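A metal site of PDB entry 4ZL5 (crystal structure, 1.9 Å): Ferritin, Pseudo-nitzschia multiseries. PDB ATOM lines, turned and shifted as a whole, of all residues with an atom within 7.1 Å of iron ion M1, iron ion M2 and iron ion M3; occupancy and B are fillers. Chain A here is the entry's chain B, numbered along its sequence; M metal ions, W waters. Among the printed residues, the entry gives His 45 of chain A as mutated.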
ATOM      1  N   GLN A  12      25.434  29.135   2.824  1.00  0.00           N
ATOM      2  CA  GLN A  12      25.456  28.674   4.207  1.00  0.00           C
ATOM      3  C   GLN A  12      26.744  29.076   4.873  1.00  0.00           C
ATOM      4  O   GLN A  12      26.758  29.401   6.034  1.00  0.00           O
ATOM      5  CB  GLN A  12      25.317  27.167   4.273  1.00  0.00           C
ATOM      6  CG  GLN A  12      25.145  26.639   5.669  1.00  0.00           C
ATOM      7  CD  GLN A  12      23.871  27.161   6.333  1.00  0.00           C
ATOM      8  OE1 GLN A  12      22.865  27.416   5.649  1.00  0.00           O
ATOM      9  NE2 GLN A  12      23.921  27.336   7.620  1.00  0.00           N
ATOM     10  N   GLN A  15      26.391  32.585   5.840  1.00  0.00           N
ATOM     11  CA  GLN A  15      25.531  32.675   6.985  1.00  0.00           C
ATOM     12  C   GLN A  15      26.313  32.360   8.271  1.00  0.00           C
ATOM     13  O   GLN A  15      26.082  33.027   9.247  1.00  0.00           O
ATOM     14  CB  GLN A  15      24.312  31.739   6.825  1.00  0.00           C
ATOM     15  CG  GLN A  15      23.296  31.733   7.935  1.00  0.00           C
ATOM     16  CD  GLN A  15      22.662  33.121   8.158  1.00  0.00           C
ATOM     17  OE1 GLN A  15      22.458  33.872   7.164  1.00  0.00           O
ATOM     18  NE2 GLN A  15      22.379  33.494   9.462  1.00  0.00           N
ATOM     19  N   GLU A  16      27.154  31.337   8.246  1.00  0.00           N
ATOM     20  CA  GLU A  16      27.911  30.987   9.451  1.00  0.00           C
ATOM     21  C   GLU A  16      28.891  32.075   9.807  1.00  0.00           C
ATOM     22  O   GLU A  16      28.990  32.418  10.981  1.00  0.00           O
ATOM     23  CB  GLU A  16      28.690  29.683   9.248  1.00  0.00           C
ATOM     24  CG  GLU A  16      27.856  28.469   8.945  1.00  0.00           C
ATOM     25  CD  GLU A  16      26.886  28.138  10.081  1.00  0.00           C
ATOM     26  OE1 GLU A  16      27.153  28.520  11.226  1.00  0.00           O
ATOM     27  OE2 GLU A  16      25.838  27.537   9.782  1.00  0.00           O
ATOM     28  N   ALA A  19      26.901  35.008  11.155  1.00  0.00           N
ATOM     29  CA  ALA A  19      26.570  34.751  12.562  1.00  0.00           C
ATOM     30  C   ALA A  19      27.774  34.922  13.464  1.00  0.00           C
ATOM     31  O   ALA A  19      27.626  35.506  14.554  1.00  0.00           O
ATOM     32  CB  ALA A  19      25.952  33.362  12.744  1.00  0.00           C
ATOM     33  N   TYR A  23      27.640  37.397  16.700  1.00  0.00           N
ATOM     34  CA  TYR A  23      28.005  37.005  18.047  1.00  0.00           C
ATOM     35  C   TYR A  23      29.140  37.847  18.570  1.00  0.00           C
ATOM     36  O   TYR A  23      29.155  38.216  19.762  1.00  0.00           O
ATOM     37  CB  TYR A  23      28.397  35.521  18.084  1.00  0.00           C
ATOM     38  CG  TYR A  23      27.269  34.557  18.237  1.00  0.00           C
ATOM     39  CD1 TYR A  23      26.694  34.313  19.457  1.00  0.00           C
ATOM     40  CD2 TYR A  23      26.793  33.816  17.174  1.00  0.00           C
ATOM     41  CE1 TYR A  23      25.680  33.384  19.620  1.00  0.00           C
ATOM     42  CE2 TYR A  23      25.714  32.935  17.323  1.00  0.00           C
ATOM     43  CZ  TYR A  23      25.198  32.725  18.569  1.00  0.00           C
ATOM     44  OH  TYR A  23      24.234  31.828  18.849  1.00  0.00           O
ATOM     45  N   HIS A  45      30.864  31.494  21.246  1.00  0.00           N
ATOM     46  CA  HIS A  45      29.943  31.058  20.305  1.00  0.00           C
ATOM     47  C   HIS A  45      30.339  31.685  18.923  1.00  0.00           C
ATOM     48  O   HIS A  45      30.162  31.046  17.925  1.00  0.00           O
ATOM     49  CB  HIS A  45      28.530  31.386  20.718  1.00  0.00           C
ATOM     50  CG  HIS A  45      27.516  30.507  20.081  1.00  0.00           C
ATOM     51  ND1 HIS A  45      26.463  29.941  20.766  1.00  0.00           N
ATOM     52  CD2 HIS A  45      27.383  30.075  18.790  1.00  0.00           C
ATOM     53  CE1 HIS A  45      25.700  29.252  19.928  1.00  0.00           C
ATOM     54  NE2 HIS A  45      26.267  29.276  18.735  1.00  0.00           N
ATOM     55  N   GLU A  48      32.766  29.378  17.484  1.00  0.00           N
ATOM     56  CA  GLU A  48      32.133  28.155  17.089  1.00  0.00           C
ATOM     57  C   GLU A  48      31.344  28.299  15.763  1.00  0.00           C
ATOM     58  O   GLU A  48      31.352  27.360  14.905  1.00  0.00           O
ATOM     59  CB  GLU A  48      31.165  27.723  18.197  1.00  0.00           C
ATOM     60  CG  GLU A  48      30.183  26.655  17.740  1.00  0.00           C
ATOM     61  CD  GLU A  48      29.286  26.196  18.887  1.00  0.00           C
ATOM     62  OE1 GLU A  48      29.646  26.455  20.057  1.00  0.00           O
ATOM     63  OE2 GLU A  48      28.212  25.610  18.602  1.00  0.00           O
ATOM     64  N   GLU A  49      30.711  29.438  15.566  1.00  0.00           N
ATOM     65  CA  GLU A  49      30.090  29.651  14.214  1.00  0.00           C
ATOM     66  C   GLU A  49      31.116  29.655  13.091  1.00  0.00           C
ATOM     67  O   GLU A  49      30.877  29.166  11.976  1.00  0.00           O
ATOM     68  CB  GLU A  49      29.371  30.939  14.133  1.00  0.00           C
ATOM     69  CG  GLU A  49      28.238  31.104  15.052  1.00  0.00           C
ATOM     70  CD  GLU A  49      27.107  30.120  14.834  1.00  0.00           C
ATOM     71  OE1 GLU A  49      26.901  29.512  13.794  1.00  0.00           O
ATOM     72  OE2 GLU A  49      26.372  30.098  15.754  1.00  0.00           O
ATOM     73  N   ARG A  50      32.248  30.306  13.351  1.00  0.00           N
ATOM     74  CA  ARG A  50      33.327  30.310  12.395  1.00  0.00           C
ATOM     75  C   ARG A  50      33.741  28.861  12.126  1.00  0.00           C
ATOM     76  O   ARG A  50      33.983  28.460  10.971  1.00  0.00           O
ATOM     77  CB  ARG A  50      34.540  31.093  12.877  1.00  0.00           C
ATOM     78  CG  ARG A  50      35.618  31.165  11.807  1.00  0.00           C
ATOM     79  CD  ARG A  50      36.583  32.357  11.957  1.00  0.00           C
ATOM     80  NE  ARG A  50      37.669  32.297  10.972  1.00  0.00           N
ATOM     81  CZ  ARG A  50      38.709  31.479  11.124  1.00  0.00           C
ATOM     82  NH1 ARG A  50      38.794  30.681  12.155  1.00  0.00           N
ATOM     83  NH2 ARG A  50      39.601  31.349  10.173  1.00  0.00           N
ATOM     84  N   HIS A  52      31.873  26.164  12.253  1.00  0.00           N
ATOM     85  CA  HIS A  52      30.864  25.595  11.374  1.00  0.00           C
ATOM     86  C   HIS A  52      31.100  26.005   9.913  1.00  0.00           C
ATOM     87  O   HIS A  52      31.025  25.174   8.987  1.00  0.00           O
ATOM     88  CB  HIS A  52      29.453  26.005  11.732  1.00  0.00           C
ATOM     89  CG  HIS A  52      29.041  25.660  13.110  1.00  0.00           C
ATOM     90  ND1 HIS A  52      29.598  24.606  13.805  1.00  0.00           N
ATOM     91  CD2 HIS A  52      28.091  26.201  13.908  1.00  0.00           C
ATOM     92  CE1 HIS A  52      29.038  24.546  14.994  1.00  0.00           C
ATOM     93  NE2 HIS A  52      28.121  25.497  15.083  1.00  0.00           N
ATOM     94  N   GLY A  53      31.332  27.283   9.695  1.00  0.00           N
ATOM     95  CA  GLY A  53      31.638  27.702   8.340  1.00  0.00           C
ATOM     96  C   GLY A  53      32.818  26.966   7.738  1.00  0.00           C
ATOM     97  O   GLY A  53      32.773  26.578   6.570  1.00  0.00           O
ATOM     98  N   PHE A  56      31.878  23.520   6.579  1.00  0.00           N
ATOM     99  CA  PHE A  56      31.263  23.600   5.282  1.00  0.00           C
ATOM    100  C   PHE A  56      32.216  23.793   4.154  1.00  0.00           C
ATOM    101  O   PHE A  56      32.099  23.100   3.151  1.00  0.00           O
ATOM    102  CB  PHE A  56      30.166  24.647   5.229  1.00  0.00           C
ATOM    103  CG  PHE A  56      28.837  24.169   5.845  1.00  0.00           C
ATOM    104  CD1 PHE A  56      28.685  24.098   7.224  1.00  0.00           C
ATOM    105  CD2 PHE A  56      27.783  23.782   5.050  1.00  0.00           C
ATOM    106  CE1 PHE A  56      27.524  23.600   7.806  1.00  0.00           C
ATOM    107  CE2 PHE A  56      26.606  23.282   5.627  1.00  0.00           C
ATOM    108  CZ  PHE A  56      26.482  23.197   7.001  1.00  0.00           C
ATOM    109  N   LEU A  94      18.853  35.042  15.162  1.00  0.00           N
ATOM    110  CA  LEU A  94      19.960  34.647  14.333  1.00  0.00           C
ATOM    111  C   LEU A  94      20.034  33.113  14.157  1.00  0.00           C
ATOM    112  O   LEU A  94      20.168  32.574  13.049  1.00  0.00           O
ATOM    113  CB  LEU A  94      21.209  35.183  15.029  1.00  0.00           C
ATOM    114  CG  LEU A  94      22.558  34.833  14.384  1.00  0.00           C
ATOM    115  CD1 LEU A  94      22.660  35.546  13.091  1.00  0.00           C
ATOM    116  CD2 LEU A  94      23.740  35.221  15.257  1.00  0.00           C
ATOM    117  N   GLU A  95      19.945  32.414  15.281  1.00  0.00           N
ATOM    118  CA  GLU A  95      19.933  30.968  15.239  1.00  0.00           C
ATOM    119  C   GLU A  95      18.729  30.405  14.567  1.00  0.00           C
ATOM    120  O   GLU A  95      18.844  29.410  13.831  1.00  0.00           O
ATOM    121  CB  GLU A  95      20.100  30.368  16.624  1.00  0.00           C
ATOM    122  CG  GLU A  95      21.509  30.521  17.231  1.00  0.00           C
ATOM    123  CD  GLU A  95      22.618  29.789  16.520  1.00  0.00           C
ATOM    124  OE1 GLU A  95      22.427  29.013  15.562  1.00  0.00           O
ATOM    125  OE2 GLU A  95      23.759  29.969  17.008  1.00  0.00           O
ATOM    126  N   ASN A  98      19.686  30.687  11.088  1.00  0.00           N
ATOM    127  CA  ASN A  98      20.722  29.677  10.784  1.00  0.00           C
ATOM    128  C   ASN A  98      19.923  28.351  10.488  1.00  0.00           C
ATOM    129  O   ASN A  98      20.137  27.670   9.457  1.00  0.00           O
ATOM    130  CB  ASN A  98      21.765  29.397  11.916  1.00  0.00           C
ATOM    131  CG  ASN A  98      22.851  30.522  12.165  1.00  0.00           C
ATOM    132  OD1 ASN A  98      23.070  31.443  11.354  1.00  0.00           O
ATOM    133  ND2 ASN A  98      23.543  30.416  13.349  1.00  0.00           N
ATOM    134  N   LEU A 102      19.715  26.038   7.024  1.00  0.00           N
ATOM    135  CA  LEU A 102      20.132  24.610   6.910  1.00  0.00           C
ATOM    136  C   LEU A 102      19.079  23.756   6.365  1.00  0.00           C
ATOM    137  O   LEU A 102      19.351  22.783   5.661  1.00  0.00           O
ATOM    138  CB  LEU A 102      20.480  23.990   8.256  1.00  0.00           C
ATOM    139  CG  LEU A 102      21.834  24.370   8.799  1.00  0.00           C
ATOM    140  CD1 LEU A 102      21.900  23.805  10.218  1.00  0.00           C
ATOM    141  CD2 LEU A 102      22.975  23.805   7.971  1.00  0.00           C
ATOM    142  N   PHE A 124      24.524  18.819  12.050  1.00  0.00           N
ATOM    143  CA  PHE A 124      24.164  20.221  12.154  1.00  0.00           C
ATOM    144  C   PHE A 124      22.661  20.415  12.434  1.00  0.00           C
ATOM    145  O   PHE A 124      22.291  21.302  13.223  1.00  0.00           O
ATOM    146  CB  PHE A 124      24.563  20.976  10.888  1.00  0.00           C
ATOM    147  CG  PHE A 124      26.042  20.979  10.618  1.00  0.00           C
ATOM    148  CD1 PHE A 124      26.867  21.933  11.249  1.00  0.00           C
ATOM    149  CD2 PHE A 124      26.629  20.054   9.761  1.00  0.00           C
ATOM    150  CE1 PHE A 124      28.222  21.960  11.011  1.00  0.00           C
ATOM    151  CE2 PHE A 124      27.993  20.095   9.484  1.00  0.00           C
ATOM    152  CZ  PHE A 124      28.798  21.009  10.143  1.00  0.00           C
ATOM    153  N   GLN A 127      22.489  19.794  16.073  1.00  0.00           N
ATOM    154  CA  GLN A 127      23.139  20.840  16.864  1.00  0.00           C
ATOM    155  C   GLN A 127      22.220  22.073  16.945  1.00  0.00           C
ATOM    156  O   GLN A 127      22.123  22.684  18.035  1.00  0.00           O
ATOM    157  CB  GLN A 127      24.457  21.262  16.233  1.00  0.00           C
ATOM    158  CG  GLN A 127      25.080  22.495  16.930  1.00  0.00           C
ATOM    159  CD  GLN A 127      26.594  22.587  16.777  1.00  0.00           C
ATOM    160  OE1 GLN A 127      27.260  23.325  17.524  1.00  0.00           O
ATOM    161  NE2 GLN A 127      27.158  21.839  15.817  1.00  0.00           N
ATOM    162  N   GLN A 128      21.545  22.384  15.854  1.00  0.00           N
ATOM    163  CA  GLN A 128      20.659  23.563  15.778  1.00  0.00           C
ATOM    164  C   GLN A 128      19.505  23.366  16.785  1.00  0.00           C
ATOM    165  O   GLN A 128      19.146  24.332  17.497  1.00  0.00           O
ATOM    166  CB  GLN A 128      20.112  23.876  14.388  1.00  0.00           C
ATOM    167  CG  GLN A 128      21.122  24.562  13.481  1.00  0.00           C
ATOM    168  CD  GLN A 128      21.741  25.777  14.163  1.00  0.00           C
ATOM    169  OE1 GLN A 128      22.890  25.725  14.654  1.00  0.00           O
ATOM    170  NE2 GLN A 128      20.914  26.801  14.378  1.00  0.00           N
ATOM    171  N   GLU A 131      21.033  24.175  20.148  1.00  0.00           N
ATOM    172  CA  GLU A 131      21.312  25.611  20.284  1.00  0.00           C
ATOM    173  C   GLU A 131      20.105  26.455  20.478  1.00  0.00           C
ATOM    174  O   GLU A 131      20.117  27.294  21.368  1.00  0.00           O
ATOM    175  CB  GLU A 131      22.119  26.141  19.070  1.00  0.00           C
ATOM    176  CG  GLU A 131      23.512  25.583  19.187  1.00  0.00           C
ATOM    177  CD  GLU A 131      24.500  26.151  18.156  1.00  0.00           C
ATOM    178  OE1 GLU A 131      24.152  27.172  17.578  1.00  0.00           O
ATOM    179  OE2 GLU A 131      25.547  25.506  17.916  1.00  0.00           O
ATOM    180  N   ILE A 135      19.570  28.730  23.836  1.00  0.00           N
ATOM    181  CA  ILE A 135      19.472  30.198  23.766  1.00  0.00           C
ATOM    182  C   ILE A 135      18.043  30.644  24.164  1.00  0.00           C
ATOM    183  O   ILE A 135      17.845  31.657  24.824  1.00  0.00           O
ATOM    184  CB  ILE A 135      19.848  30.700  22.358  1.00  0.00           C
ATOM    185  CG1 ILE A 135      21.285  30.316  22.039  1.00  0.00           C
ATOM    186  CG2 ILE A 135      19.610  32.182  22.220  1.00  0.00           C
ATOM    187  CD1 ILE A 135      21.577  30.356  20.560  1.00  0.00           C
HETATM  188 FE    FE M   1      25.369  28.536  16.680  1.00  0.00          FE
HETATM  189 FE    FE M   2      26.655  25.268  16.464  1.00  0.00          FE
HETATM  190 FE    FE M   3      26.011  27.928  13.043  1.00  0.00          FE
HETATM  191  O   HOH W   1      25.075  26.093  11.983  1.00  0.00           O
HETATM  192  O   HOH W   2      24.570  27.696  14.815  1.00  0.00           O
HETATM  193  O   HOH W   3      26.994  27.408  16.851  1.00  0.00           O
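Water W2 lies within hydrogen-bond range of the side-chain amide oxygen (OE1) of Gln 128 (2.6 Å), the side-chain carboxylate (OE1) of Glu 95 (2.6 Å) and the side-chain amide nitrogen (ND2) of Asn 98 (3.3 Å). Water W1 bridges the side-chain carboxylate of Glu 16 (2.7 Å) and the side-chain amide oxygen of Gln 128 (3.5 Å).
OE1 of Glu 49 is bound to iron ion M3, at 2.0 Å. Iron ion M3 is bound by OE1 of Glu 16 (2.2 Å). Water W2 binds iron ion M3. Water W1 is bound to iron ion M3, 2.3 Å away.
Asn 98 touches iron ion M3 (ND2 to FE, 3.5 Å). Of the 21 residues printed, 4 come within 4 Å of iron ion M3. The nearest printed residue that does not touch iron ion M3 is Gln 128 (4.1 Å).
Within 4 Å of iron ion M1: His 45, Glu 49, Glu 95 and Glu 131.
Iron ion M1 is bound by water W3 (2.0 Å). Iron ion M1 is bound by OE1 of Glu 131, 2.0 Å away. OE2 of Glu 49 binds iron ion M1, 2.1 Å away. OE2 of Glu 95 binds iron ion M1 (2.2 Å). Water W2 is bound to iron ion M1 (2.2 Å). Iron ion M1 is bound by NE2 of His 45, at 2.4 Å.
The side-chain amide oxygen (OE1) of Gln 128 lies close to the side-chain carboxylate (OE1) of Glu 131 (3.5 Å). The backbone carbonyl oxygen of Glu 48 lies close to a ring nitrogen (ND1) of His 52. OE1 of Glu 95 is in hydrogen-bond range of ND2 of Asn 98 (2.8 Å). The side-chain hydroxyl (OH) of Tyr 23 lies close to the side-chain carboxylate (OE2) of Glu 95, at 2.7 Å. The side-chain amide nitrogen (NE2) of Gln 128 is in hydrogen-bond range of the side-chain carboxylate (OE1) of Glu 95, at 2.9 Å. OE2 of Glu 16 sits at hydrogen-bond distance from NE2 of Gln 12 (2.9 Å). The side-chain amide oxygen of Gln 127 lies close to the side-chain carboxylate of Glu 48, at 2.7 Å. The side-chain amide nitrogen (NE2) of Gln 15 sits at hydrogen-bond distance from the side-chain amide oxygen (OD1) of Asn 98, at 2.9 Å.
Iron ion M2 is bound by the side-chain carboxylate (OE2) of Glu 131, a ring nitrogen (NE2) of His 52, water W3 and the side-chain amide oxygen (OE1) of Gln 127. Iron ion M2 has four donor atoms within binding distance. Slightly farther from iron ion M2 lies OE2 of Glu 48 (2.7 Å).
Within 4 Å of iron ion M2: Glu 48, His 52, Gln 127 and Glu 131. The nearest printed residue that does not touch iron ion M2 is Gln 128 (4.2 Å).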
